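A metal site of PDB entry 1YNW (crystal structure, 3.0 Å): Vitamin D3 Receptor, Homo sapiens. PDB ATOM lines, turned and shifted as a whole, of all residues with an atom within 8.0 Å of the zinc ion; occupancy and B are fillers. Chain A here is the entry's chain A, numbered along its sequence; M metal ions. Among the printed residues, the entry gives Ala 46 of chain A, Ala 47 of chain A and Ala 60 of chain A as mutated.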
ATOM      1  N   THR A  44     -13.796  30.989  11.917  1.00  0.00           N
ATOM      2  CA  THR A  44     -14.725  30.748  10.805  1.00  0.00           C
ATOM      3  C   THR A  44     -15.365  29.375  11.040  1.00  0.00           C
ATOM      4  O   THR A  44     -14.694  28.344  11.146  1.00  0.00           O
ATOM      5  CB  THR A  44     -14.017  30.784   9.440  1.00  0.00           C
ATOM      6  OG1 THR A  44     -13.025  29.752   9.400  1.00  0.00           O
ATOM      7  CG2 THR A  44     -13.313  32.122   9.234  1.00  0.00           C
ATOM      8  N   CYS A  45     -16.679  29.385  11.151  1.00  0.00           N
ATOM      9  CA  CYS A  45     -17.454  28.194  11.434  1.00  0.00           C
ATOM     10  C   CYS A  45     -17.569  27.240  10.254  1.00  0.00           C
ATOM     11  O   CYS A  45     -18.067  27.629   9.198  1.00  0.00           O
ATOM     12  CB  CYS A  45     -18.835  28.660  11.909  1.00  0.00           C
ATOM     13  SG  CYS A  45     -20.234  27.745  11.328  1.00  0.00           S
ATOM     14  N   ALA A  46     -17.118  25.988  10.413  1.00  0.00           N
ATOM     15  CA  ALA A  46     -17.226  25.018   9.304  1.00  0.00           C
ATOM     16  C   ALA A  46     -18.681  24.943   8.847  1.00  0.00           C
ATOM     17  O   ALA A  46     -18.973  25.119   7.674  1.00  0.00           O
ATOM     18  CB  ALA A  46     -16.731  23.624   9.723  1.00  0.00           C
ATOM     19  N   ALA A  47     -19.592  24.685   9.781  1.00  0.00           N
ATOM     20  CA  ALA A  47     -21.006  24.582   9.455  1.00  0.00           C
ATOM     21  C   ALA A  47     -21.536  25.788   8.679  1.00  0.00           C
ATOM     22  O   ALA A  47     -20.778  26.496   8.013  1.00  0.00           O
ATOM     23  CB  ALA A  47     -21.832  24.379  10.735  1.00  0.00           C
ATOM     24  N   ASN A  48     -22.832  26.012   8.772  1.00  0.00           N
ATOM     25  CA  ASN A  48     -23.442  27.134   8.069  1.00  0.00           C
ATOM     26  C   ASN A  48     -23.650  28.286   9.023  1.00  0.00           C
ATOM     27  O   ASN A  48     -24.735  28.904   9.070  1.00  0.00           O
ATOM     28  CB  ASN A  48     -24.771  26.731   7.411  1.00  0.00           C
ATOM     29  CG  ASN A  48     -24.579  26.226   5.975  1.00  0.00           C
ATOM     30  OD1 ASN A  48     -24.338  27.026   5.062  1.00  0.00           O
ATOM     31  ND2 ASN A  48     -24.658  24.908   5.777  1.00  0.00           N
ATOM     32  N   GLY A  49     -22.577  28.549   9.779  1.00  0.00           N
ATOM     33  CA  GLY A  49     -22.538  29.628  10.752  1.00  0.00           C
ATOM     34  C   GLY A  49     -23.733  29.716  11.668  1.00  0.00           C
ATOM     35  O   GLY A  49     -24.386  30.766  11.731  1.00  0.00           O
ATOM     36  N   ASP A  50     -24.023  28.637  12.391  1.00  0.00           N
ATOM     37  CA  ASP A  50     -25.155  28.712  13.286  1.00  0.00           C
ATOM     38  C   ASP A  50     -25.350  27.577  14.263  1.00  0.00           C
ATOM     39  O   ASP A  50     -26.483  27.183  14.566  1.00  0.00           O
ATOM     40  CB  ASP A  50     -26.434  28.919  12.482  1.00  0.00           C
ATOM     41  CG  ASP A  50     -27.520  29.569  13.324  1.00  0.00           C
ATOM     42  OD1 ASP A  50     -27.198  30.560  14.042  1.00  0.00           O
ATOM     43  OD2 ASP A  50     -28.676  29.090  13.261  1.00  0.00           O
ATOM     44  N   CYS A  51     -24.241  27.058  14.767  1.00  0.00           N
ATOM     45  CA  CYS A  51     -24.326  25.973  15.739  1.00  0.00           C
ATOM     46  C   CYS A  51     -24.966  26.512  17.035  1.00  0.00           C
ATOM     47  O   CYS A  51     -25.108  27.735  17.208  1.00  0.00           O
ATOM     48  CB  CYS A  51     -22.919  25.424  16.065  1.00  0.00           C
ATOM     49  SG  CYS A  51     -21.571  26.054  14.998  1.00  0.00           S
ATOM     50  N   ARG A  52     -25.377  25.605  17.910  1.00  0.00           N
ATOM     51  CA  ARG A  52     -25.954  25.993  19.201  1.00  0.00           C
ATOM     52  C   ARG A  52     -24.908  25.753  20.299  1.00  0.00           C
ATOM     53  O   ARG A  52     -24.399  24.627  20.487  1.00  0.00           O
ATOM     54  CB  ARG A  52     -27.241  25.220  19.510  1.00  0.00           C
ATOM     55  CG  ARG A  52     -28.380  25.661  18.639  1.00  0.00           C
ATOM     56  CD  ARG A  52     -29.721  25.104  19.072  1.00  0.00           C
ATOM     57  NE  ARG A  52     -30.707  25.303  18.011  1.00  0.00           N
ATOM     58  CZ  ARG A  52     -31.964  24.844  18.036  1.00  0.00           C
ATOM     59  NH1 ARG A  52     -32.406  24.159  19.090  1.00  0.00           N
ATOM     60  NH2 ARG A  52     -32.777  25.070  17.007  1.00  0.00           N
ATOM     61  N   ILE A  53     -24.582  26.836  20.994  1.00  0.00           N
ATOM     62  CA  ILE A  53     -23.592  26.793  22.068  1.00  0.00           C
ATOM     63  C   ILE A  53     -24.212  26.147  23.310  1.00  0.00           C
ATOM     64  O   ILE A  53     -25.321  26.499  23.731  1.00  0.00           O
ATOM     65  CB  ILE A  53     -23.114  28.227  22.417  1.00  0.00           C
ATOM     66  CG1 ILE A  53     -22.844  29.028  21.131  1.00  0.00           C
ATOM     67  CG2 ILE A  53     -21.849  28.143  23.292  1.00  0.00           C
ATOM     68  CD1 ILE A  53     -21.629  28.583  20.316  1.00  0.00           C
ATOM     69  N   ALA A  60     -16.435  23.457  20.462  1.00  0.00           N
ATOM     70  CA  ALA A  60     -16.556  22.871  19.116  1.00  0.00           C
ATOM     71  C   ALA A  60     -16.311  23.900  18.043  1.00  0.00           C
ATOM     72  O   ALA A  60     -15.302  23.818  17.352  1.00  0.00           O
ATOM     73  CB  ALA A  60     -17.922  22.290  18.933  1.00  0.00           C
ATOM     74  N   CYS A  61     -17.240  24.854  17.907  1.00  0.00           N
ATOM     75  CA  CYS A  61     -17.156  25.926  16.885  1.00  0.00           C
ATOM     76  C   CYS A  61     -16.855  27.326  17.487  1.00  0.00           C
ATOM     77  O   CYS A  61     -17.769  28.061  17.899  1.00  0.00           O
ATOM     78  CB  CYS A  61     -18.475  25.961  16.094  1.00  0.00           C
ATOM     79  SG  CYS A  61     -18.486  27.012  14.627  1.00  0.00           S
ATOM     80  N   GLN A  62     -15.584  27.711  17.533  1.00  0.00           N
ATOM     81  CA  GLN A  62     -15.198  29.011  18.085  1.00  0.00           C
ATOM     82  C   GLN A  62     -15.902  30.157  17.383  1.00  0.00           C
ATOM     83  O   GLN A  62     -16.580  30.966  18.012  1.00  0.00           O
ATOM     84  CB  GLN A  62     -13.691  29.211  17.980  1.00  0.00           C
ATOM     85  CG  GLN A  62     -12.890  28.127  18.706  1.00  0.00           C
ATOM     86  CD  GLN A  62     -11.395  28.304  18.525  1.00  0.00           C
ATOM     87  OE1 GLN A  62     -10.888  28.421  17.421  1.00  0.00           O
ATOM     88  NE2 GLN A  62     -10.680  28.323  19.625  1.00  0.00           N
ATOM     89  N   ALA A  63     -15.749  30.243  16.081  1.00  0.00           N
ATOM     90  CA  ALA A  63     -16.417  31.319  15.384  1.00  0.00           C
ATOM     91  C   ALA A  63     -17.824  31.585  15.950  1.00  0.00           C
ATOM     92  O   ALA A  63     -18.181  32.737  16.251  1.00  0.00           O
ATOM     93  CB  ALA A  63     -16.489  31.003  13.902  1.00  0.00           C
ATOM     94  N   CYS A  64     -18.638  30.560  16.113  1.00  0.00           N
ATOM     95  CA  CYS A  64     -19.983  30.818  16.609  1.00  0.00           C
ATOM     96  C   CYS A  64     -19.995  31.292  18.077  1.00  0.00           C
ATOM     97  O   CYS A  64     -20.746  32.225  18.406  1.00  0.00           O
ATOM     98  CB  CYS A  64     -20.879  29.571  16.435  1.00  0.00           C
ATOM     99  SG  CYS A  64     -21.775  29.392  14.786  1.00  0.00           S
ATOM    100  N   ARG A  65     -19.177  30.671  18.931  1.00  0.00           N
ATOM    101  CA  ARG A  65     -19.084  31.056  20.354  1.00  0.00           C
ATOM    102  C   ARG A  65     -18.841  32.548  20.399  1.00  0.00           C
ATOM    103  O   ARG A  65     -19.655  33.318  20.950  1.00  0.00           O
ATOM    104  CB  ARG A  65     -17.905  30.353  21.059  1.00  0.00           C
ATOM    105  CG  ARG A  65     -17.861  30.538  22.602  1.00  0.00           C
ATOM    106  CD  ARG A  65     -16.736  29.696  23.272  1.00  0.00           C
ATOM    107  NE  ARG A  65     -16.869  29.635  24.736  1.00  0.00           N
ATOM    108  CZ  ARG A  65     -16.014  29.002  25.545  1.00  0.00           C
ATOM    109  NH1 ARG A  65     -14.948  28.367  25.038  1.00  0.00           N
ATOM    110  NH2 ARG A  65     -16.186  29.008  26.855  1.00  0.00           N
ATOM    111  N   LYS A  67     -19.080  34.938  18.075  1.00  0.00           N
ATOM    112  CA  LYS A  67     -20.203  35.712  17.555  1.00  0.00           C
ATOM    113  C   LYS A  67     -21.340  35.765  18.565  1.00  0.00           C
ATOM    114  O   LYS A  67     -22.054  36.776  18.676  1.00  0.00           O
ATOM    115  CB  LYS A  67     -20.746  35.122  16.251  1.00  0.00           C
ATOM    116  CG  LYS A  67     -21.958  35.880  15.705  1.00  0.00           C
ATOM    117  CD  LYS A  67     -22.841  34.919  14.887  1.00  0.00           C
ATOM    118  CE  LYS A  67     -24.226  35.497  14.566  1.00  0.00           C
ATOM    119  NZ  LYS A  67     -25.222  34.441  14.222  1.00  0.00           N
HETATM  120 ZN    ZN M   1     -20.564  27.652  13.729  1.00  0.00          ZN
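SG of Cys 51 is bound to the zinc ion, 2.3 Å away. The zinc ion is bound by SG of Cys 61, at 2.4 Å. The zinc ion is bound by the side-chain sulfur (SG) of Cys 64 (2.4 Å). The zinc ion is bound by SG of Cys 45, 2.4 Å away.
The side-chain sulfur (SG) of Cys 64 sits close to the backbone NH (N) of Asp 50 (3.4 Å). The side-chain sulfur of Cys 45 lies close to the backbone NH of Gly 49 (2.9 Å). The backbone NH (N) of Ala 47 sits close to the side-chain sulfur (SG) of Cys 45, 3.5 Å away.
Merely in contact with the zinc ion: Asp 50 (3.8 Å). The nearest printed residue that does not touch the zinc ion is Gly 49 (4.1 Å).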
